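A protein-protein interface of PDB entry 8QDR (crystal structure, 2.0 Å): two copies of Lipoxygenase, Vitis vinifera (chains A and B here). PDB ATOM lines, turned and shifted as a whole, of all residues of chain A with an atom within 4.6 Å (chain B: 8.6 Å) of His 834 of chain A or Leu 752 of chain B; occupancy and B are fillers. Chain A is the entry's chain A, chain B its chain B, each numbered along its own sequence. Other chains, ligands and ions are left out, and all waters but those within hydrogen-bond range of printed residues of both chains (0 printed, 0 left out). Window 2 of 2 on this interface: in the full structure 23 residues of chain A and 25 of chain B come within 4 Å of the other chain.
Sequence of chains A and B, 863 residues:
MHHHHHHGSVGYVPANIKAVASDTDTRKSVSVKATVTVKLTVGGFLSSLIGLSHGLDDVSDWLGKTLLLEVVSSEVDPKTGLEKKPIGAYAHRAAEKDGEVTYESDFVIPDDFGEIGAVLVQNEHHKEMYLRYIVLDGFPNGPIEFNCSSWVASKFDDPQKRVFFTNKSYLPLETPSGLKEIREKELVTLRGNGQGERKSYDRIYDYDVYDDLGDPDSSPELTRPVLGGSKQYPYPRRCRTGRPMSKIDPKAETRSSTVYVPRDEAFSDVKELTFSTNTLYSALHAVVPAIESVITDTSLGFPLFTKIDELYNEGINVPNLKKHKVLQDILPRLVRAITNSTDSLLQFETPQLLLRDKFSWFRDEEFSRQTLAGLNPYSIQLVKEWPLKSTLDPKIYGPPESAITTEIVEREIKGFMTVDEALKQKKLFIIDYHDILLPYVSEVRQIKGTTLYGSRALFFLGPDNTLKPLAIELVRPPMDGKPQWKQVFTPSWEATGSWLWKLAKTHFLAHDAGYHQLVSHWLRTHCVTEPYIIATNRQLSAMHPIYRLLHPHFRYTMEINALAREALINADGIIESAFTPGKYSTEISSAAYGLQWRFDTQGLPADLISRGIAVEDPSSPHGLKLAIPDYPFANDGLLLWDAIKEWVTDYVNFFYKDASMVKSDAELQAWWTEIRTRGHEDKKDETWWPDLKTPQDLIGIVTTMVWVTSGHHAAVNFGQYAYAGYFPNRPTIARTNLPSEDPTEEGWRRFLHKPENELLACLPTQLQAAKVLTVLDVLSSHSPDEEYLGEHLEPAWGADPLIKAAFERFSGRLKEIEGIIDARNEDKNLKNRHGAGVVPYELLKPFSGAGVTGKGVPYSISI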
ATOM      1  N   ASN A 825      17.157  -0.045 -16.092  1.00  0.00           N
ATOM      2  CA  ASN A 825      17.840   0.501 -17.252  1.00  0.00           C
ATOM      3  C   ASN A 825      18.556   1.800 -16.948  1.00  0.00           C
ATOM      4  O   ASN A 825      19.296   2.270 -17.809  1.00  0.00           O
ATOM      5  CB  ASN A 825      16.859   0.702 -18.404  1.00  0.00           C
ATOM      6  CG  ASN A 825      16.487  -0.619 -19.079  1.00  0.00           C
ATOM      7  OD1 ASN A 825      17.293  -1.553 -19.109  1.00  0.00           O
ATOM      8  ND2 ASN A 825      15.281  -0.698 -19.628  1.00  0.00           N
ATOM      9  N   GLU A 826      18.377   2.377 -15.756  1.00  0.00           N
ATOM     10  CA  GLU A 826      19.166   3.526 -15.315  1.00  0.00           C
ATOM     11  C   GLU A 826      20.211   3.175 -14.260  1.00  0.00           C
ATOM     12  O   GLU A 826      20.897   4.074 -13.775  1.00  0.00           O
ATOM     13  CB  GLU A 826      18.256   4.636 -14.760  1.00  0.00           C
ATOM     14  CG  GLU A 826      17.142   5.060 -15.694  1.00  0.00           C
ATOM     15  CD  GLU A 826      17.646   5.670 -16.999  1.00  0.00           C
ATOM     16  OE1 GLU A 826      18.607   6.474 -16.979  1.00  0.00           O
ATOM     17  OE2 GLU A 826      17.054   5.360 -18.054  1.00  0.00           O
ATOM     18  N   ASP A 827      20.347   1.906 -13.885  1.00  0.00           N
ATOM     19  CA  ASP A 827      21.256   1.502 -12.813  1.00  0.00           C
ATOM     20  C   ASP A 827      22.674   1.385 -13.362  1.00  0.00           C
ATOM     21  O   ASP A 827      22.953   0.498 -14.173  1.00  0.00           O
ATOM     22  CB  ASP A 827      20.783   0.174 -12.223  1.00  0.00           C
ATOM     23  CG  ASP A 827      21.520  -0.208 -10.950  1.00  0.00           C
ATOM     24  OD1 ASP A 827      22.608   0.341 -10.694  1.00  0.00           O
ATOM     25  OD2 ASP A 827      20.997  -1.067 -10.206  1.00  0.00           O
ATOM     26  N   LYS A 828      23.586   2.254 -12.903  1.00  0.00           N
ATOM     27  CA  LYS A 828      24.973   2.187 -13.358  1.00  0.00           C
ATOM     28  C   LYS A 828      25.649   0.882 -12.958  1.00  0.00           C
ATOM     29  O   LYS A 828      26.656   0.513 -13.560  1.00  0.00           O
ATOM     30  CB  LYS A 828      25.781   3.372 -12.814  1.00  0.00           C
ATOM     31  CG  LYS A 828      25.851   3.386 -11.307  1.00  0.00           C
ATOM     32  CD  LYS A 828      26.843   4.407 -10.767  1.00  0.00           C
ATOM     33  CE  LYS A 828      26.871   4.354  -9.246  1.00  0.00           C
ATOM     34  NZ  LYS A 828      28.128   4.920  -8.695  1.00  0.00           N
ATOM     35  N   LEU A 830      24.325  -2.066 -13.385  1.00  0.00           N
ATOM     36  CA  LEU A 830      23.819  -3.135 -14.250  1.00  0.00           C
ATOM     37  C   LEU A 830      24.408  -2.902 -15.639  1.00  0.00           C
ATOM     38  O   LEU A 830      23.752  -2.448 -16.572  1.00  0.00           O
ATOM     39  CB  LEU A 830      22.283  -3.149 -14.229  1.00  0.00           C
ATOM     40  CG  LEU A 830      21.654  -3.500 -12.864  1.00  0.00           C
ATOM     41  CD1 LEU A 830      20.105  -3.622 -12.891  1.00  0.00           C
ATOM     42  CD2 LEU A 830      22.250  -4.813 -12.330  1.00  0.00           C
ATOM     43  N   LYS A 831      25.695  -3.233 -15.759  1.00  0.00           N
ATOM     44  CA  LYS A 831      26.450  -2.886 -16.953  1.00  0.00           C
ATOM     45  C   LYS A 831      25.997  -3.664 -18.171  1.00  0.00           C
ATOM     46  O   LYS A 831      26.356  -3.288 -19.292  1.00  0.00           O
ATOM     47  CB  LYS A 831      27.936  -3.100 -16.694  1.00  0.00           C
ATOM     48  CG  LYS A 831      28.464  -2.189 -15.597  1.00  0.00           C
ATOM     49  CD  LYS A 831      29.936  -2.398 -15.356  1.00  0.00           C
ATOM     50  CE  LYS A 831      30.447  -1.435 -14.299  1.00  0.00           C
ATOM     51  NZ  LYS A 831      31.878  -1.699 -13.960  1.00  0.00           N
ATOM     52  N   ASN A 832      25.205  -4.720 -17.992  1.00  0.00           N
ATOM     53  CA  ASN A 832      24.709  -5.440 -19.154  1.00  0.00           C
ATOM     54  C   ASN A 832      23.465  -4.793 -19.755  1.00  0.00           C
ATOM     55  O   ASN A 832      22.995  -5.241 -20.808  1.00  0.00           O
ATOM     56  CB  ASN A 832      24.468  -6.912 -18.785  1.00  0.00           C
ATOM     57  CG  ASN A 832      25.780  -7.636 -18.477  1.00  0.00           C
ATOM     58  OD1 ASN A 832      26.785  -7.459 -19.191  1.00  0.00           O
ATOM     59  ND2 ASN A 832      25.791  -8.424 -17.405  1.00  0.00           N
ATOM     60  N   ARG A 833      22.952  -3.720 -19.142  1.00  0.00           N
ATOM     61  CA  ARG A 833      21.824  -3.023 -19.733  1.00  0.00           C
ATOM     62  C   ARG A 833      21.966  -1.518 -19.709  1.00  0.00           C
ATOM     63  O   ARG A 833      21.127  -0.837 -20.306  1.00  0.00           O
ATOM     64  CB  ARG A 833      20.519  -3.421 -19.030  1.00  0.00           C
ATOM     65  CG  ARG A 833      20.423  -2.984 -17.563  1.00  0.00           C
ATOM     66  CD  ARG A 833      19.352  -3.770 -16.850  1.00  0.00           C
ATOM     67  NE  ARG A 833      18.049  -3.603 -17.485  1.00  0.00           N
ATOM     68  CZ  ARG A 833      17.002  -4.391 -17.256  1.00  0.00           C
ATOM     69  NH1 ARG A 833      17.106  -5.420 -16.430  1.00  0.00           N
ATOM     70  NH2 ARG A 833      15.859  -4.168 -17.879  1.00  0.00           N
ATOM     71  N   HIS A 834      23.006  -0.981 -19.075  1.00  0.00           N
ATOM     72  CA  HIS A 834      23.215   0.457 -18.930  1.00  0.00           C
ATOM     73  C   HIS A 834      24.688   0.763 -19.171  1.00  0.00           C
ATOM     74  O   HIS A 834      25.551   0.213 -18.479  1.00  0.00           O
ATOM     75  CB  HIS A 834      22.781   0.892 -17.529  1.00  0.00           C
ATOM     76  CG  HIS A 834      22.980   2.340 -17.233  1.00  0.00           C
ATOM     77  ND1 HIS A 834      24.135   2.830 -16.657  1.00  0.00           N
ATOM     78  CD2 HIS A 834      22.143   3.397 -17.352  1.00  0.00           C
ATOM     79  CE1 HIS A 834      24.009   4.130 -16.460  1.00  0.00           C
ATOM     80  NE2 HIS A 834      22.811   4.498 -16.879  1.00  0.00           N
ATOM     81  N   GLY A 835      24.972   1.632 -20.134  1.00  0.00           N
ATOM     82  CA  GLY A 835      26.347   2.007 -20.425  1.00  0.00           C
ATOM     83  C   GLY A 835      26.422   2.815 -21.701  1.00  0.00           C
ATOM     84  O   GLY A 835      25.427   3.007 -22.406  1.00  0.00           O
ATOM     85  N   ALA A 836      27.641   3.289 -21.990  1.00  0.00           N
ATOM     86  CA  ALA A 836      27.846   4.179 -23.127  1.00  0.00           C
ATOM     87  C   ALA A 836      27.407   3.499 -24.419  1.00  0.00           C
ATOM     88  O   ALA A 836      27.970   2.473 -24.820  1.00  0.00           O
ATOM     89  CB  ALA A 836      29.316   4.609 -23.208  1.00  0.00           C
ATOM     90  N   GLY A 837      26.408   4.077 -25.085  1.00  0.00           N
ATOM     91  CA  GLY A 837      25.917   3.478 -26.308  1.00  0.00           C
ATOM     92  C   GLY A 837      25.149   2.187 -26.136  1.00  0.00           C
ATOM     93  O   GLY A 837      24.848   1.530 -27.135  1.00  0.00           O
ATOM     94  N   VAL A 838      24.816   1.798 -24.909  1.00  0.00           N
ATOM     95  CA  VAL A 838      24.043   0.583 -24.660  1.00  0.00           C
ATOM     96  C   VAL A 838      22.559   0.908 -24.758  1.00  0.00           C
ATOM     97  O   VAL A 838      22.053   1.773 -24.037  1.00  0.00           O
ATOM     98  CB  VAL A 838      24.376  -0.018 -23.288  1.00  0.00           C
ATOM     99  CG1 VAL A 838      23.497  -1.237 -23.019  1.00  0.00           C
ATOM    100  CG2 VAL A 838      25.829  -0.414 -23.235  1.00  0.00           C
ATOM    101  N   GLU B 494      33.565  -3.926 -21.350  1.00  0.00           N
ATOM    102  CA  GLU B 494      32.235  -3.375 -21.110  1.00  0.00           C
ATOM    103  C   GLU B 494      32.165  -2.014 -21.789  1.00  0.00           C
ATOM    104  O   GLU B 494      33.194  -1.370 -22.034  1.00  0.00           O
ATOM    105  CB  GLU B 494      31.888  -3.295 -19.601  1.00  0.00           C
ATOM    106  CG  GLU B 494      32.866  -2.550 -18.717  1.00  0.00           C
ATOM    107  CD  GLU B 494      32.548  -1.057 -18.598  1.00  0.00           C
ATOM    108  OE1 GLU B 494      31.500  -0.616 -19.118  1.00  0.00           O
ATOM    109  OE2 GLU B 494      33.354  -0.326 -17.982  1.00  0.00           O
ATOM    110  N   ALA B 495      30.947  -1.583 -22.112  1.00  0.00           N
ATOM    111  CA  ALA B 495      30.786  -0.523 -23.109  1.00  0.00           C
ATOM    112  C   ALA B 495      31.387   0.808 -22.649  1.00  0.00           C
ATOM    113  O   ALA B 495      32.103   1.473 -23.410  1.00  0.00           O
ATOM    114  CB  ALA B 495      29.310  -0.365 -23.458  1.00  0.00           C
ATOM    115  N   THR B 496      31.108   1.222 -21.413  1.00  0.00           N
ATOM    116  CA  THR B 496      31.587   2.529 -20.965  1.00  0.00           C
ATOM    117  C   THR B 496      33.111   2.568 -20.896  1.00  0.00           C
ATOM    118  O   THR B 496      33.735   3.511 -21.398  1.00  0.00           O
ATOM    119  CB  THR B 496      30.983   2.888 -19.608  1.00  0.00           C
ATOM    120  OG1 THR B 496      29.555   2.934 -19.713  1.00  0.00           O
ATOM    121  CG2 THR B 496      31.502   4.266 -19.151  1.00  0.00           C
ATOM    122  N   GLY B 497      33.731   1.553 -20.278  1.00  0.00           N
ATOM    123  CA  GLY B 497      35.187   1.515 -20.223  1.00  0.00           C
ATOM    124  C   GLY B 497      35.824   1.476 -21.596  1.00  0.00           C
ATOM    125  O   GLY B 497      36.906   2.036 -21.809  1.00  0.00           O
ATOM    126  N   TRP B 499      34.474   2.817 -24.380  1.00  0.00           N
ATOM    127  CA  TRP B 499      34.311   4.148 -24.963  1.00  0.00           C
ATOM    128  C   TRP B 499      35.280   5.148 -24.348  1.00  0.00           C
ATOM    129  O   TRP B 499      35.826   6.004 -25.057  1.00  0.00           O
ATOM    130  CB  TRP B 499      32.859   4.627 -24.803  1.00  0.00           C
ATOM    131  CG  TRP B 499      32.060   4.304 -26.019  1.00  0.00           C
ATOM    132  CD1 TRP B 499      31.141   3.307 -26.161  1.00  0.00           C
ATOM    133  CD2 TRP B 499      32.167   4.939 -27.299  1.00  0.00           C
ATOM    134  NE1 TRP B 499      30.643   3.303 -27.441  1.00  0.00           N
ATOM    135  CE2 TRP B 499      31.261   4.292 -28.160  1.00  0.00           C
ATOM    136  CE3 TRP B 499      32.933   6.002 -27.796  1.00  0.00           C
ATOM    137  CZ2 TRP B 499      31.096   4.674 -29.491  1.00  0.00           C
ATOM    138  CZ3 TRP B 499      32.763   6.383 -29.119  1.00  0.00           C
ATOM    139  CH2 TRP B 499      31.849   5.722 -29.947  1.00  0.00           C
ATOM    140  N   LEU B 500      35.501   5.067 -23.032  1.00  0.00           N
ATOM    141  CA  LEU B 500      36.508   5.929 -22.410  1.00  0.00           C
ATOM    142  C   LEU B 500      37.913   5.628 -22.939  1.00  0.00           C
ATOM    143  O   LEU B 500      38.736   6.545 -23.101  1.00  0.00           O
ATOM    144  CB  LEU B 500      36.439   5.773 -20.889  1.00  0.00           C
ATOM    145  CG  LEU B 500      35.150   6.337 -20.272  1.00  0.00           C
ATOM    146  CD1 LEU B 500      35.033   6.004 -18.779  1.00  0.00           C
ATOM    147  CD2 LEU B 500      35.066   7.843 -20.526  1.00  0.00           C
ATOM    148  N   PRO B 739      34.772  12.711 -20.975  1.00  0.00           N
ATOM    149  CA  PRO B 739      33.478  12.817 -20.275  1.00  0.00           C
ATOM    150  C   PRO B 739      33.578  12.539 -18.788  1.00  0.00           C
ATOM    151  O   PRO B 739      32.772  13.063 -18.012  1.00  0.00           O
ATOM    152  CB  PRO B 739      32.609  11.771 -20.989  1.00  0.00           C
ATOM    153  CG  PRO B 739      33.248  11.599 -22.328  1.00  0.00           C
ATOM    154  CD  PRO B 739      34.713  11.745 -22.082  1.00  0.00           C
ATOM    155  N   GLU B 745      25.804  15.556 -14.019  1.00  0.00           N
ATOM    156  CA  GLU B 745      24.870  14.450 -14.187  1.00  0.00           C
ATOM    157  C   GLU B 745      24.339  14.401 -15.616  1.00  0.00           C
ATOM    158  O   GLU B 745      24.308  13.334 -16.240  1.00  0.00           O
ATOM    159  CB  GLU B 745      23.726  14.550 -13.169  1.00  0.00           C
ATOM    160  CG  GLU B 745      23.992  13.753 -11.888  1.00  0.00           C
ATOM    161  CD  GLU B 745      22.915  13.920 -10.825  1.00  0.00           C
ATOM    162  OE1 GLU B 745      23.226  13.688  -9.636  1.00  0.00           O
ATOM    163  OE2 GLU B 745      21.763  14.280 -11.168  1.00  0.00           O
ATOM    164  N   GLU B 746      23.977  15.554 -16.175  1.00  0.00           N
ATOM    165  CA  GLU B 746      23.392  15.555 -17.508  1.00  0.00           C
ATOM    166  C   GLU B 746      24.423  15.524 -18.626  1.00  0.00           C
ATOM    167  O   GLU B 746      24.104  15.054 -19.725  1.00  0.00           O
ATOM    168  CB  GLU B 746      22.482  16.770 -17.692  1.00  0.00           C
ATOM    169  CG  GLU B 746      23.177  18.095 -17.553  1.00  0.00           C
ATOM    170  CD  GLU B 746      22.350  19.221 -18.136  1.00  0.00           C
ATOM    171  OE1 GLU B 746      21.720  18.997 -19.192  1.00  0.00           O
ATOM    172  OE2 GLU B 746      22.317  20.317 -17.537  1.00  0.00           O
ATOM    173  N   GLY B 747      25.645  16.010 -18.391  1.00  0.00           N
ATOM    174  CA  GLY B 747      26.695  15.818 -19.382  1.00  0.00           C
ATOM    175  C   GLY B 747      27.074  14.355 -19.516  1.00  0.00           C
ATOM    176  O   GLY B 747      27.255  13.846 -20.626  1.00  0.00           O
ATOM    177  N   TRP B 748      27.167  13.657 -18.381  1.00  0.00           N
ATOM    178  CA  TRP B 748      27.440  12.227 -18.387  1.00  0.00           C
ATOM    179  C   TRP B 748      26.331  11.455 -19.091  1.00  0.00           C
ATOM    180  O   TRP B 748      26.609  10.501 -19.824  1.00  0.00           O
ATOM    181  CB  TRP B 748      27.623  11.723 -16.953  1.00  0.00           C
ATOM    182  CG  TRP B 748      28.044  10.282 -16.878  1.00  0.00           C
ATOM    183  CD1 TRP B 748      27.299   9.218 -16.437  1.00  0.00           C
ATOM    184  CD2 TRP B 748      29.307   9.751 -17.271  1.00  0.00           C
ATOM    185  NE1 TRP B 748      28.035   8.059 -16.525  1.00  0.00           N
ATOM    186  CE2 TRP B 748      29.268   8.360 -17.042  1.00  0.00           C
ATOM    187  CE3 TRP B 748      30.475  10.320 -17.798  1.00  0.00           C
ATOM    188  CZ2 TRP B 748      30.346   7.534 -17.321  1.00  0.00           C
ATOM    189  CZ3 TRP B 748      31.546   9.495 -18.074  1.00  0.00           C
ATOM    190  CH2 TRP B 748      31.477   8.124 -17.833  1.00  0.00           C
ATOM    191  N   ARG B 749      25.069  11.855 -18.897  1.00  0.00           N
ATOM    192  CA  ARG B 749      23.974  11.113 -19.527  1.00  0.00           C
ATOM    193  C   ARG B 749      23.959  11.336 -21.037  1.00  0.00           C
ATOM    194  O   ARG B 749      23.637  10.420 -21.808  1.00  0.00           O
ATOM    195  CB  ARG B 749      22.623  11.489 -18.907  1.00  0.00           C
ATOM    196  CG  ARG B 749      21.497  10.555 -19.352  1.00  0.00           C
ATOM    197  CD  ARG B 749      20.099  11.039 -18.974  1.00  0.00           C
ATOM    198  NE  ARG B 749      19.724  10.674 -17.613  1.00  0.00           N
ATOM    199  CZ  ARG B 749      19.565  11.554 -16.632  1.00  0.00           C
ATOM    200  NH1 ARG B 749      19.735  12.848 -16.872  1.00  0.00           N
ATOM    201  NH2 ARG B 749      19.223  11.148 -15.418  1.00  0.00           N
ATOM    202  N   ARG B 750      24.318  12.538 -21.479  1.00  0.00           N
ATOM    203  CA  ARG B 750      24.433  12.788 -22.909  1.00  0.00           C
ATOM    204  C   ARG B 750      25.522  11.920 -23.535  1.00  0.00           C
ATOM    205  O   ARG B 750      25.359  11.417 -24.656  1.00  0.00           O
ATOM    206  CB  ARG B 750      24.704  14.276 -23.146  1.00  0.00           C
ATOM    207  CG  ARG B 750      24.976  14.670 -24.584  1.00  0.00           C
ATOM    208  CD  ARG B 750      25.093  16.183 -24.713  1.00  0.00           C
ATOM    209  NE  ARG B 750      23.905  16.884 -24.217  1.00  0.00           N
ATOM    210  CZ  ARG B 750      23.864  17.611 -23.100  1.00  0.00           C
ATOM    211  NH1 ARG B 750      24.949  17.744 -22.349  1.00  0.00           N
ATOM    212  NH2 ARG B 750      22.738  18.214 -22.735  1.00  0.00           N
ATOM    213  N   PHE B 751      26.639  11.726 -22.825  1.00  0.00           N
ATOM    214  CA  PHE B 751      27.701  10.867 -23.347  1.00  0.00           C
ATOM    215  C   PHE B 751      27.249   9.411 -23.434  1.00  0.00           C
ATOM    216  O   PHE B 751      27.526   8.730 -24.426  1.00  0.00           O
ATOM    217  CB  PHE B 751      28.954  10.996 -22.480  1.00  0.00           C
ATOM    218  CG  PHE B 751      29.923   9.836 -22.614  1.00  0.00           C
ATOM    219  CD1 PHE B 751      30.558   9.573 -23.822  1.00  0.00           C
ATOM    220  CD2 PHE B 751      30.235   9.044 -21.516  1.00  0.00           C
ATOM    221  CE1 PHE B 751      31.459   8.523 -23.934  1.00  0.00           C
ATOM    222  CE2 PHE B 751      31.144   7.985 -21.626  1.00  0.00           C
ATOM    223  CZ  PHE B 751      31.749   7.729 -22.834  1.00  0.00           C
ATOM    224  N   LEU B 752      26.554   8.915 -22.407  1.00  0.00           N
ATOM    225  CA  LEU B 752      26.063   7.542 -22.459  1.00  0.00           C
ATOM    226  C   LEU B 752      25.083   7.352 -23.608  1.00  0.00           C
ATOM    227  O   LEU B 752      25.084   6.306 -24.262  1.00  0.00           O
ATOM    228  CB  LEU B 752      25.406   7.145 -21.138  1.00  0.00           C
ATOM    229  CG  LEU B 752      26.297   7.149 -19.895  1.00  0.00           C
ATOM    230  CD1 LEU B 752      25.525   6.635 -18.683  1.00  0.00           C
ATOM    231  CD2 LEU B 752      27.553   6.345 -20.124  1.00  0.00           C
ATOM    232  N   HIS B 753      24.266   8.362 -23.894  1.00  0.00           N
ATOM    233  CA  HIS B 753      23.216   8.183 -24.892  1.00  0.00           C
ATOM    234  C   HIS B 753      23.771   8.214 -26.311  1.00  0.00           C
ATOM    235  O   HIS B 753      23.332   7.433 -27.163  1.00  0.00           O
ATOM    236  CB  HIS B 753      22.141   9.259 -24.719  1.00  0.00           C
ATOM    237  CG  HIS B 753      20.914   9.038 -25.554  1.00  0.00           C
ATOM    238  ND1 HIS B 753      20.222  10.073 -26.148  1.00  0.00           N
ATOM    239  CD2 HIS B 753      20.241   7.906 -25.875  1.00  0.00           C
ATOM    240  CE1 HIS B 753      19.185   9.588 -26.808  1.00  0.00           C
ATOM    241  NE2 HIS B 753      19.173   8.276 -26.658  1.00  0.00           N
ATOM    242  N   LYS B 754      24.712   9.119 -26.593  1.00  0.00           N
ATOM    243  CA  LYS B 754      25.299   9.252 -27.929  1.00  0.00           C
ATOM    244  C   LYS B 754      26.806   9.454 -27.813  1.00  0.00           C
ATOM    245  O   LYS B 754      27.323  10.568 -27.980  1.00  0.00           O
ATOM    246  CB  LYS B 754      24.638  10.396 -28.702  1.00  0.00           C
ATOM    247  CG  LYS B 754      23.116  10.443 -28.576  1.00  0.00           C
ATOM    248  CD  LYS B 754      22.450  11.156 -29.741  1.00  0.00           C
ATOM    249  CE  LYS B 754      22.293  10.237 -30.946  1.00  0.00           C
ATOM    250  NZ  LYS B 754      21.443  10.864 -31.997  1.00  0.00           N
ATOM    251  N   PRO B 755      27.554   8.379 -27.538  1.00  0.00           N
ATOM    252  CA  PRO B 755      29.015   8.524 -27.411  1.00  0.00           C
ATOM    253  C   PRO B 755      29.698   8.800 -28.737  1.00  0.00           C
ATOM    254  O   PRO B 755      30.780   9.396 -28.750  1.00  0.00           O
ATOM    255  CB  PRO B 755      29.449   7.177 -26.815  1.00  0.00           C
ATOM    256  CG  PRO B 755      28.421   6.218 -27.311  1.00  0.00           C
ATOM    257  CD  PRO B 755      27.120   6.990 -27.311  1.00  0.00           C
ATOM    258  N   GLU B 756      29.084   8.392 -29.850  1.00  0.00           N
ATOM    259  CA  GLU B 756      29.588   8.749 -31.173  1.00  0.00           C
ATOM    260  C   GLU B 756      29.623  10.265 -31.364  1.00  0.00           C
ATOM    261  O   GLU B 756      30.550  10.801 -31.980  1.00  0.00           O
ATOM    262  CB  GLU B 756      28.717   8.091 -32.243  1.00  0.00           C
ATOM    263  CG  GLU B 756      29.212   8.275 -33.658  1.00  0.00           C
ATOM    264  CD  GLU B 756      30.145   7.165 -34.099  1.00  0.00           C
ATOM    265  OE1 GLU B 756      29.859   5.985 -33.789  1.00  0.00           O
ATOM    266  OE2 GLU B 756      31.163   7.475 -34.759  1.00  0.00           O
ATOM    267  N   GLU B 758      30.036  12.454 -28.969  1.00  0.00           N
ATOM    268  CA  GLU B 758      31.132  12.951 -28.149  1.00  0.00           C
ATOM    269  C   GLU B 758      32.466  12.732 -28.847  1.00  0.00           C
ATOM    270  O   GLU B 758      33.341  13.610 -28.831  1.00  0.00           O
ATOM    271  CB  GLU B 758      31.104  12.270 -26.778  1.00  0.00           C
ATOM    272  CG  GLU B 758      32.208  12.708 -25.836  1.00  0.00           C
ATOM    273  CD  GLU B 758      32.211  14.210 -25.576  1.00  0.00           C
ATOM    274  OE1 GLU B 758      31.156  14.748 -25.171  1.00  0.00           O
ATOM    275  OE2 GLU B 758      33.269  14.850 -25.782  1.00  0.00           O
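The backbone NH (N) of Ala 836 of chain A lies within hydrogen-bond range of the side-chain hydroxyl (OG1) of Thr 496 of chain B (3.0 Å).
The backbone NH of Gly 837 of chain A sits at hydrogen-bond distance from the backbone carbonyl oxygen of Leu 752 of chain B, 2.7 Å away.
The backbone NH (N) of Thr 496 of chain B sits at hydrogen-bond distance from the side-chain carboxylate (OE1) of Glu 494 of chain B (3.0 Å).
Among the printed residues, merely in contact across the chains: His 834 of chain A with Leu 752 of chain B (3.7 Å), Gly 835 of chain A with Thr 496 of chain B (3.4 Å), Gly 835 of chain A with Leu 752 of chain B (3.8 Å), Ala 836 of chain A with Ala 495 of chain B (3.4 Å), Ala 836 of chain A with Trp 499 of chain B (3.5 Å), Ala 836 of chain A with Phe 751 of chain B (3.97 Å), Ala 836 of chain A with Leu 752 of chain B (3.6 Å), Gly 837 of chain A with Pro 755 of chain B (3.7 Å) and Val 838 of chain A with Ala 495 of chain B (3.5 Å).
His 834 of chain A touches just one residue of chain B: Leu 752 (3.7 Å).
Gly 835 of chain A touches just these residues of chain B: Thr 496 and Leu 752.
Printed residues of chain B within 4 Å of Ala 836 of chain A: Ala 495, Thr 496, Trp 499, Phe 751 and Leu 752.
Printed residues of chain B within 4 Å of Val 838 of chain A: Ala 495.
Of the printed residues of chain A, Thr 496 of chain B touches Gly 835 and Ala 836.
Of the printed residues of chain A, Trp 499 of chain B touches Ala 836 (3.5 Å).
Glu 745 of chain B touches none of the printed residues of chain A.
Printed residues of chain A within 4 Å of Phe 751 of chain B: Ala 836 (3.97 Å).
Leu 752 of chain B touches just these residues of chain A: His 834 (3.7 Å), Gly 835 (3.8 Å), Ala 836 (3.6 Å) and Gly 837 (2.7 Å).
The nearest printed residue of chain A that does not touch Phe 751 of chain B is Gly 837 of chain A (4.8 Å).
Of the 20 printed residues of chain B, 6 touch a printed residue of chain A.
Hydrophobic or aromatic side chains of chain B within 4 Å of the printed part of chain A: Ala 495, Trp 499, Phe 751, Leu 752 and Pro 755.
Along chain B the printed residues that touch a printed residue of chain A span positions 495 to 755.
Hydrophobic or aromatic side chains of chain A within 4 Å of the printed part of chain B: His 834, Ala 836 and Val 838.
Among the printed residues, 11 pairs touch across the chains.
No position is printed for both chains.
Of the 11 pairs that touch across the chains among the printed residues, none has its exchanged pair printed and touching as well.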
